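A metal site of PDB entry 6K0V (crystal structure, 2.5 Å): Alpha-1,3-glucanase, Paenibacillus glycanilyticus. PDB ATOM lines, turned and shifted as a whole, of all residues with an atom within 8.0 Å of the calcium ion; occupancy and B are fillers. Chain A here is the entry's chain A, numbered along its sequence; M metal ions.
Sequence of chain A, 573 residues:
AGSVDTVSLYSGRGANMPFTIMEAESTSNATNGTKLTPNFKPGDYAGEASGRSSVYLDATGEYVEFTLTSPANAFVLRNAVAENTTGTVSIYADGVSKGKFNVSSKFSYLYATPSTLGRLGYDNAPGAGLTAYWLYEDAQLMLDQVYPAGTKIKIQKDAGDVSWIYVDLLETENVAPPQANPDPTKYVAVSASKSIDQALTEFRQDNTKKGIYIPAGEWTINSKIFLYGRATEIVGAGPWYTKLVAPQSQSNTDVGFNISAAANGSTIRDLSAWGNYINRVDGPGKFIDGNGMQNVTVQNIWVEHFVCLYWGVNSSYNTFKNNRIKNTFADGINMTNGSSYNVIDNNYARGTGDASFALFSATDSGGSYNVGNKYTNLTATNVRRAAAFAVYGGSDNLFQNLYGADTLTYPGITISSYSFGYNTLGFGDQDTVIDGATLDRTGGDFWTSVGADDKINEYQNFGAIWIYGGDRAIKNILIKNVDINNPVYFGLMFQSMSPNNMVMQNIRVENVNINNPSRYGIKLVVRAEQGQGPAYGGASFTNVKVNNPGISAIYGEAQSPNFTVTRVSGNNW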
ATOM      1  N   ILE A  21       3.962 -14.575  11.647  1.00  0.00           N
ATOM      2  CA  ILE A  21       3.899 -14.038  13.004  1.00  0.00           C
ATOM      3  C   ILE A  21       4.940 -14.722  13.864  1.00  0.00           C
ATOM      4  O   ILE A  21       4.975 -15.948  13.947  1.00  0.00           O
ATOM      5  CB  ILE A  21       2.508 -14.216  13.622  1.00  0.00           C
ATOM      6  CG1 ILE A  21       1.431 -13.667  12.687  1.00  0.00           C
ATOM      7  CG2 ILE A  21       2.445 -13.486  14.932  1.00  0.00           C
ATOM      8  CD1 ILE A  21       0.112 -13.652  13.319  1.00  0.00           C
ATOM      9  N   MET A  22       5.772 -13.925  14.523  1.00  0.00           N
ATOM     10  CA  MET A  22       6.772 -14.450  15.431  1.00  0.00           C
ATOM     11  C   MET A  22       6.545 -13.933  16.834  1.00  0.00           C
ATOM     12  O   MET A  22       6.442 -12.720  17.033  1.00  0.00           O
ATOM     13  CB  MET A  22       8.157 -14.069  14.942  1.00  0.00           C
ATOM     14  CG  MET A  22       8.304 -14.383  13.483  1.00  0.00           C
ATOM     15  SD  MET A  22      10.001 -14.267  12.958  1.00  0.00           S
ATOM     16  CE  MET A  22       9.877 -15.201  11.426  1.00  0.00           C
ATOM     17  N   GLU A  23       6.448 -14.826  17.810  1.00  0.00           N
ATOM     18  CA  GLU A  23       6.213 -14.382  19.169  1.00  0.00           C
ATOM     19  C   GLU A  23       7.500 -13.828  19.757  1.00  0.00           C
ATOM     20  O   GLU A  23       8.582 -14.383  19.543  1.00  0.00           O
ATOM     21  CB  GLU A  23       5.674 -15.513  20.047  1.00  0.00           C
ATOM     22  CG  GLU A  23       4.336 -16.088  19.608  1.00  0.00           C
ATOM     23  CD  GLU A  23       3.166 -15.160  19.909  1.00  0.00           C
ATOM     24  OE1 GLU A  23       3.387 -14.056  20.446  1.00  0.00           O
ATOM     25  OE2 GLU A  23       2.023 -15.539  19.618  1.00  0.00           O
ATOM     26  N   ALA A  24       7.394 -12.694  20.450  1.00  0.00           N
ATOM     27  CA  ALA A  24       8.606 -12.091  20.985  1.00  0.00           C
ATOM     28  C   ALA A  24       9.253 -12.991  22.036  1.00  0.00           C
ATOM     29  O   ALA A  24      10.480 -13.170  22.023  1.00  0.00           O
ATOM     30  CB  ALA A  24       8.326 -10.698  21.540  1.00  0.00           C
ATOM     31  N   GLU A  25       8.461 -13.603  22.915  1.00  0.00           N
ATOM     32  CA  GLU A  25       8.961 -14.386  24.037  1.00  0.00           C
ATOM     33  C   GLU A  25       9.571 -15.719  23.617  1.00  0.00           C
ATOM     34  O   GLU A  25      10.054 -16.446  24.495  1.00  0.00           O
ATOM     35  CB  GLU A  25       7.844 -14.673  25.023  1.00  0.00           C
ATOM     36  CG  GLU A  25       6.800 -15.568  24.416  1.00  0.00           C
ATOM     37  CD  GLU A  25       5.742 -14.779  23.667  1.00  0.00           C
ATOM     38  OE1 GLU A  25       4.624 -15.312  23.531  1.00  0.00           O
ATOM     39  OE2 GLU A  25       6.006 -13.632  23.216  1.00  0.00           O
ATOM     40  N   SER A  26       9.514 -16.085  22.351  1.00  0.00           N
ATOM     41  CA  SER A  26      10.102 -17.347  21.944  1.00  0.00           C
ATOM     42  C   SER A  26      11.562 -17.386  22.365  1.00  0.00           C
ATOM     43  O   SER A  26      12.312 -16.417  22.191  1.00  0.00           O
ATOM     44  CB  SER A  26       9.973 -17.516  20.429  1.00  0.00           C
ATOM     45  OG  SER A  26      11.073 -18.240  19.889  1.00  0.00           O
ATOM     46  N   LYS A  35      10.997 -11.526  30.029  1.00  0.00           N
ATOM     47  CA  LYS A  35       9.920 -12.380  29.551  1.00  0.00           C
ATOM     48  C   LYS A  35       8.902 -12.612  30.680  1.00  0.00           C
ATOM     49  O   LYS A  35       9.246 -13.160  31.732  1.00  0.00           O
ATOM     50  CB  LYS A  35      10.470 -13.695  29.012  1.00  0.00           C
ATOM     51  CG  LYS A  35       9.435 -14.486  28.220  1.00  0.00           C
ATOM     52  CD  LYS A  35       9.771 -15.966  28.107  1.00  0.00           C
ATOM     53  CE  LYS A  35       8.698 -16.820  28.808  1.00  0.00           C
ATOM     54  NZ  LYS A  35       7.369 -16.927  28.097  1.00  0.00           N
ATOM     55  N   TYR A  45      -0.709  -7.731  31.196  1.00  0.00           N
ATOM     56  CA  TYR A  45       0.107  -7.678  30.003  1.00  0.00           C
ATOM     57  C   TYR A  45       0.490  -9.051  29.493  1.00  0.00           C
ATOM     58  O   TYR A  45       0.751  -9.191  28.300  1.00  0.00           O
ATOM     59  CB  TYR A  45       1.343  -6.823  30.259  1.00  0.00           C
ATOM     60  CG  TYR A  45       0.975  -5.369  30.428  1.00  0.00           C
ATOM     61  CD1 TYR A  45       0.657  -4.580  29.328  1.00  0.00           C
ATOM     62  CD2 TYR A  45       0.905  -4.793  31.690  1.00  0.00           C
ATOM     63  CE1 TYR A  45       0.296  -3.238  29.488  1.00  0.00           C
ATOM     64  CE2 TYR A  45       0.554  -3.456  31.869  1.00  0.00           C
ATOM     65  CZ  TYR A  45       0.254  -2.681  30.777  1.00  0.00           C
ATOM     66  OH  TYR A  45      -0.098  -1.355  30.964  1.00  0.00           O
ATOM     67  N   ALA A  46       0.527 -10.077  30.333  1.00  0.00           N
ATOM     68  CA  ALA A  46       0.693 -11.405  29.769  1.00  0.00           C
ATOM     69  C   ALA A  46      -0.654 -11.967  29.321  1.00  0.00           C
ATOM     70  O   ALA A  46      -0.785 -12.473  28.192  1.00  0.00           O
ATOM     71  CB  ALA A  46       1.374 -12.349  30.761  1.00  0.00           C
ATOM     72  N   GLU A  48      -3.243 -10.607  28.196  1.00  0.00           N
ATOM     73  CA  GLU A  48      -3.755 -10.008  26.969  1.00  0.00           C
ATOM     74  C   GLU A  48      -2.845 -10.190  25.765  1.00  0.00           C
ATOM     75  O   GLU A  48      -3.191  -9.747  24.673  1.00  0.00           O
ATOM     76  CB  GLU A  48      -4.029  -8.525  27.195  1.00  0.00           C
ATOM     77  CG  GLU A  48      -5.103  -8.263  28.231  1.00  0.00           C
ATOM     78  CD  GLU A  48      -5.871  -6.995  27.926  1.00  0.00           C
ATOM     79  OE1 GLU A  48      -5.505  -6.312  26.925  1.00  0.00           O
ATOM     80  OE2 GLU A  48      -6.824  -6.695  28.675  1.00  0.00           O
ATOM     81  N   ALA A  49      -1.708 -10.842  25.939  1.00  0.00           N
ATOM     82  CA  ALA A  49      -0.732 -10.995  24.872  1.00  0.00           C
ATOM     83  C   ALA A  49      -0.986 -12.270  24.060  1.00  0.00           C
ATOM     84  O   ALA A  49      -1.640 -13.217  24.503  1.00  0.00           O
ATOM     85  CB  ALA A  49       0.704 -10.995  25.432  1.00  0.00           C
ATOM     86  N   SER A  50      -0.457 -12.261  22.836  1.00  0.00           N
ATOM     87  CA  SER A  50      -0.470 -13.448  22.001  1.00  0.00           C
ATOM     88  C   SER A  50       0.454 -14.517  22.576  1.00  0.00           C
ATOM     89  O   SER A  50       1.624 -14.257  22.826  1.00  0.00           O
ATOM     90  CB  SER A  50      -0.045 -13.085  20.586  1.00  0.00           C
ATOM     91  OG  SER A  50      -0.121 -14.210  19.731  1.00  0.00           O
ATOM     92  N   GLY A  51      -0.063 -15.739  22.757  1.00  0.00           N
ATOM     93  CA  GLY A  51       0.731 -16.725  23.459  1.00  0.00           C
ATOM     94  C   GLY A  51       0.828 -16.475  24.948  1.00  0.00           C
ATOM     95  O   GLY A  51       1.676 -17.073  25.619  1.00  0.00           O
ATOM     96  N   ARG A  52      -0.011 -15.584  25.469  1.00  0.00           N
ATOM     97  CA  ARG A  52      -0.075 -15.239  26.873  1.00  0.00           C
ATOM     98  C   ARG A  52       1.270 -14.793  27.452  1.00  0.00           C
ATOM     99  O   ARG A  52       1.528 -14.958  28.643  1.00  0.00           O
ATOM    100  CB  ARG A  52      -0.667 -16.392  27.675  1.00  0.00           C
ATOM    101  CG  ARG A  52      -1.960 -16.907  27.105  1.00  0.00           C
ATOM    102  CD  ARG A  52      -3.092 -15.879  27.171  1.00  0.00           C
ATOM    103  NE  ARG A  52      -4.305 -16.499  26.673  1.00  0.00           N
ATOM    104  CZ  ARG A  52      -5.552 -16.175  27.027  1.00  0.00           C
ATOM    105  NH1 ARG A  52      -5.772 -15.182  27.886  1.00  0.00           N
ATOM    106  NH2 ARG A  52      -6.562 -16.869  26.528  1.00  0.00           N
ATOM    107  N   SER A  53       2.130 -14.208  26.619  1.00  0.00           N
ATOM    108  CA  SER A  53       3.395 -13.669  27.133  1.00  0.00           C
ATOM    109  C   SER A  53       3.920 -12.640  26.155  1.00  0.00           C
ATOM    110  O   SER A  53       3.472 -12.556  25.018  1.00  0.00           O
ATOM    111  CB  SER A  53       4.430 -14.783  27.376  1.00  0.00           C
ATOM    112  OG  SER A  53       5.700 -14.272  27.763  1.00  0.00           O
ATOM    113  N   SER A  54       4.880 -11.853  26.620  1.00  0.00           N
ATOM    114  CA  SER A  54       5.520 -10.812  25.838  1.00  0.00           C
ATOM    115  C   SER A  54       6.834 -10.476  26.539  1.00  0.00           C
ATOM    116  O   SER A  54       7.098 -10.943  27.645  1.00  0.00           O
ATOM    117  CB  SER A  54       4.607  -9.597  25.695  1.00  0.00           C
ATOM    118  OG  SER A  54       4.659  -8.825  26.872  1.00  0.00           O
ATOM    119  N   VAL A  55       7.670  -9.682  25.866  1.00  0.00           N
ATOM    120  CA  VAL A  55       8.975  -9.316  26.409  1.00  0.00           C
ATOM    121  C   VAL A  55       8.955  -7.837  26.779  1.00  0.00           C
ATOM    122  O   VAL A  55       8.679  -6.969  25.949  1.00  0.00           O
ATOM    123  CB  VAL A  55      10.105  -9.633  25.416  1.00  0.00           C
ATOM    124  CG1 VAL A  55      11.407  -9.211  25.990  1.00  0.00           C
ATOM    125  CG2 VAL A  55      10.135 -11.126  25.115  1.00  0.00           C
ATOM    126  N   ARG A  78       3.094  -5.744  17.509  1.00  0.00           N
ATOM    127  CA  ARG A  78       2.027  -5.682  18.509  1.00  0.00           C
ATOM    128  C   ARG A  78       2.661  -5.388  19.868  1.00  0.00           C
ATOM    129  O   ARG A  78       3.508  -6.143  20.337  1.00  0.00           O
ATOM    130  CB  ARG A  78       1.219  -6.970  18.564  1.00  0.00           C
ATOM    131  CG  ARG A  78       0.076  -6.955  19.594  1.00  0.00           C
ATOM    132  CD  ARG A  78      -0.843  -8.133  19.394  1.00  0.00           C
ATOM    133  NE  ARG A  78      -2.230  -7.894  19.793  1.00  0.00           N
ATOM    134  CZ  ARG A  78      -2.760  -8.261  20.962  1.00  0.00           C
ATOM    135  NH1 ARG A  78      -1.999  -8.848  21.857  1.00  0.00           N
ATOM    136  NH2 ARG A  78      -4.039  -8.032  21.238  1.00  0.00           N
ATOM    137  N   TYR A 136      -2.951  -3.973  24.329  1.00  0.00           N
ATOM    138  CA  TYR A 136      -2.022  -4.092  23.217  1.00  0.00           C
ATOM    139  C   TYR A 136      -2.578  -3.433  21.971  1.00  0.00           C
ATOM    140  O   TYR A 136      -3.760  -3.615  21.634  1.00  0.00           O
ATOM    141  CB  TYR A 136      -1.707  -5.559  22.933  1.00  0.00           C
ATOM    142  CG  TYR A 136      -0.753  -6.137  23.934  1.00  0.00           C
ATOM    143  CD1 TYR A 136       0.612  -5.970  23.791  1.00  0.00           C
ATOM    144  CD2 TYR A 136      -1.226  -6.798  25.050  1.00  0.00           C
ATOM    145  CE1 TYR A 136       1.493  -6.474  24.713  1.00  0.00           C
ATOM    146  CE2 TYR A 136      -0.376  -7.311  25.990  1.00  0.00           C
ATOM    147  CZ  TYR A 136       1.000  -7.141  25.818  1.00  0.00           C
ATOM    148  OH  TYR A 136       1.881  -7.648  26.759  1.00  0.00           O
ATOM    149  N   VAL A 167       6.722  -6.008  24.258  1.00  0.00           N
ATOM    150  CA  VAL A 167       6.773  -6.477  22.873  1.00  0.00           C
ATOM    151  C   VAL A 167       6.125  -7.858  22.831  1.00  0.00           C
ATOM    152  O   VAL A 167       6.640  -8.804  23.435  1.00  0.00           O
ATOM    153  CB  VAL A 167       8.203  -6.501  22.330  1.00  0.00           C
ATOM    154  CG1 VAL A 167       8.218  -7.107  20.930  1.00  0.00           C
ATOM    155  CG2 VAL A 167       8.794  -5.081  22.308  1.00  0.00           C
ATOM    156  N   ASP A 168       5.005  -7.977  22.109  1.00  0.00           N
ATOM    157  CA  ASP A 168       4.195  -9.189  22.087  1.00  0.00           C
ATOM    158  C   ASP A 168       4.588 -10.131  20.943  1.00  0.00           C
ATOM    159  O   ASP A 168       4.975 -11.279  21.165  1.00  0.00           O
ATOM    160  CB  ASP A 168       2.715  -8.828  21.988  1.00  0.00           C
ATOM    161  CG  ASP A 168       1.804 -10.048  22.065  1.00  0.00           C
ATOM    162  OD1 ASP A 168       2.304 -11.172  22.252  1.00  0.00           O
ATOM    163  OD2 ASP A 168       0.564  -9.879  21.975  1.00  0.00           O
ATOM    164  N   LEU A 169       4.455  -9.655  19.707  1.00  0.00           N
ATOM    165  CA  LEU A 169       4.848 -10.418  18.536  1.00  0.00           C
ATOM    166  C   LEU A 169       5.305  -9.446  17.465  1.00  0.00           C
ATOM    167  O   LEU A 169       5.037  -8.253  17.537  1.00  0.00           O
ATOM    168  CB  LEU A 169       3.706 -11.295  18.002  1.00  0.00           C
ATOM    169  CG  LEU A 169       2.405 -10.554  17.618  1.00  0.00           C
ATOM    170  CD1 LEU A 169       2.440  -9.901  16.202  1.00  0.00           C
ATOM    171  CD2 LEU A 169       1.205 -11.492  17.734  1.00  0.00           C
ATOM    172  N   LEU A 170       5.977  -9.982  16.448  1.00  0.00           N
ATOM    173  CA  LEU A 170       6.308  -9.229  15.246  1.00  0.00           C
ATOM    174  C   LEU A 170       5.799 -10.040  14.068  1.00  0.00           C
ATOM    175  O   LEU A 170       6.234 -11.170  13.877  1.00  0.00           O
ATOM    176  CB  LEU A 170       7.820  -9.013  15.134  1.00  0.00           C
ATOM    177  CG  LEU A 170       8.319  -8.279  13.878  1.00  0.00           C
ATOM    178  CD1 LEU A 170       8.199  -6.759  14.031  1.00  0.00           C
ATOM    179  CD2 LEU A 170       9.767  -8.696  13.519  1.00  0.00           C
ATOM    180  N   ASN A 382      -6.520 -13.491  19.802  1.00  0.00           N
ATOM    181  CA  ASN A 382      -6.528 -12.304  20.648  1.00  0.00           C
ATOM    182  C   ASN A 382      -7.902 -11.630  20.617  1.00  0.00           C
ATOM    183  O   ASN A 382      -8.032 -10.431  20.406  1.00  0.00           O
ATOM    184  CB  ASN A 382      -5.434 -11.303  20.248  1.00  0.00           C
ATOM    185  CG  ASN A 382      -4.056 -11.717  20.702  1.00  0.00           C
ATOM    186  OD1 ASN A 382      -3.199 -12.057  19.895  1.00  0.00           O
ATOM    187  ND2 ASN A 382      -3.822 -11.665  22.014  1.00  0.00           N
ATOM    188  N   ASP A 406      -6.176 -17.691  22.205  1.00  0.00           N
ATOM    189  CA  ASP A 406      -6.049 -16.577  23.139  1.00  0.00           C
ATOM    190  C   ASP A 406      -7.264 -15.643  23.045  1.00  0.00           C
ATOM    191  O   ASP A 406      -7.190 -14.492  22.634  1.00  0.00           O
ATOM    192  CB  ASP A 406      -4.748 -15.808  22.933  1.00  0.00           C
ATOM    193  CG  ASP A 406      -3.527 -16.692  23.087  1.00  0.00           C
ATOM    194  OD1 ASP A 406      -3.479 -17.459  24.066  1.00  0.00           O
ATOM    195  OD2 ASP A 406      -2.604 -16.621  22.233  1.00  0.00           O
ATOM    196  N   ARG A 441      -5.381 -22.300  23.987  1.00  0.00           N
ATOM    197  CA  ARG A 441      -5.548 -21.404  25.124  1.00  0.00           C
ATOM    198  C   ARG A 441      -6.801 -20.530  24.988  1.00  0.00           C
ATOM    199  O   ARG A 441      -6.724 -19.305  25.008  1.00  0.00           O
ATOM    200  CB  ARG A 441      -4.320 -20.522  25.293  1.00  0.00           C
ATOM    201  CG  ARG A 441      -3.022 -21.255  25.414  1.00  0.00           C
ATOM    202  CD  ARG A 441      -1.872 -20.239  25.404  1.00  0.00           C
ATOM    203  NE  ARG A 441      -1.947 -19.426  24.189  1.00  0.00           N
ATOM    204  CZ  ARG A 441      -1.483 -19.815  23.004  1.00  0.00           C
ATOM    205  NH1 ARG A 441      -0.881 -20.985  22.868  1.00  0.00           N
ATOM    206  NH2 ARG A 441      -1.637 -19.012  21.949  1.00  0.00           N
HETATM  207 CA    CA M   1       3.564 -13.095  22.695  1.00  0.00          CA
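Of the 26 residues printed, 5 come within 4 Å of the calcium ion.
The calcium ion is bound by O of Ser 50, 2.3 Å away.
OD1 of Asp 168 is bound to the calcium ion.
O of Ser 53 binds the calcium ion, at 2.4 Å.
The side-chain carboxylate (OE1) of Glu 23 is bound to the calcium ion (2.5 Å).
OE2 of Glu 25 binds the calcium ion, 2.6 Å away.
The side-chain carboxylate (OE1) of Glu 25 binds the calcium ion, at 2.6 Å.
The calcium ion is bound by O of Asp 168 (2.8 Å).
The calcium ion has seven donor atoms within binding distance.
NZ of Lys 35 lies within hydrogen-bond range of OG of Ser 53 (3.2 Å).
O of Asp 168 lies close to N of Ala 24 (2.9 Å).
OD2 of Asp 168 is in salt-bridge range of NH1 of Arg 78, at 2.8 Å.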
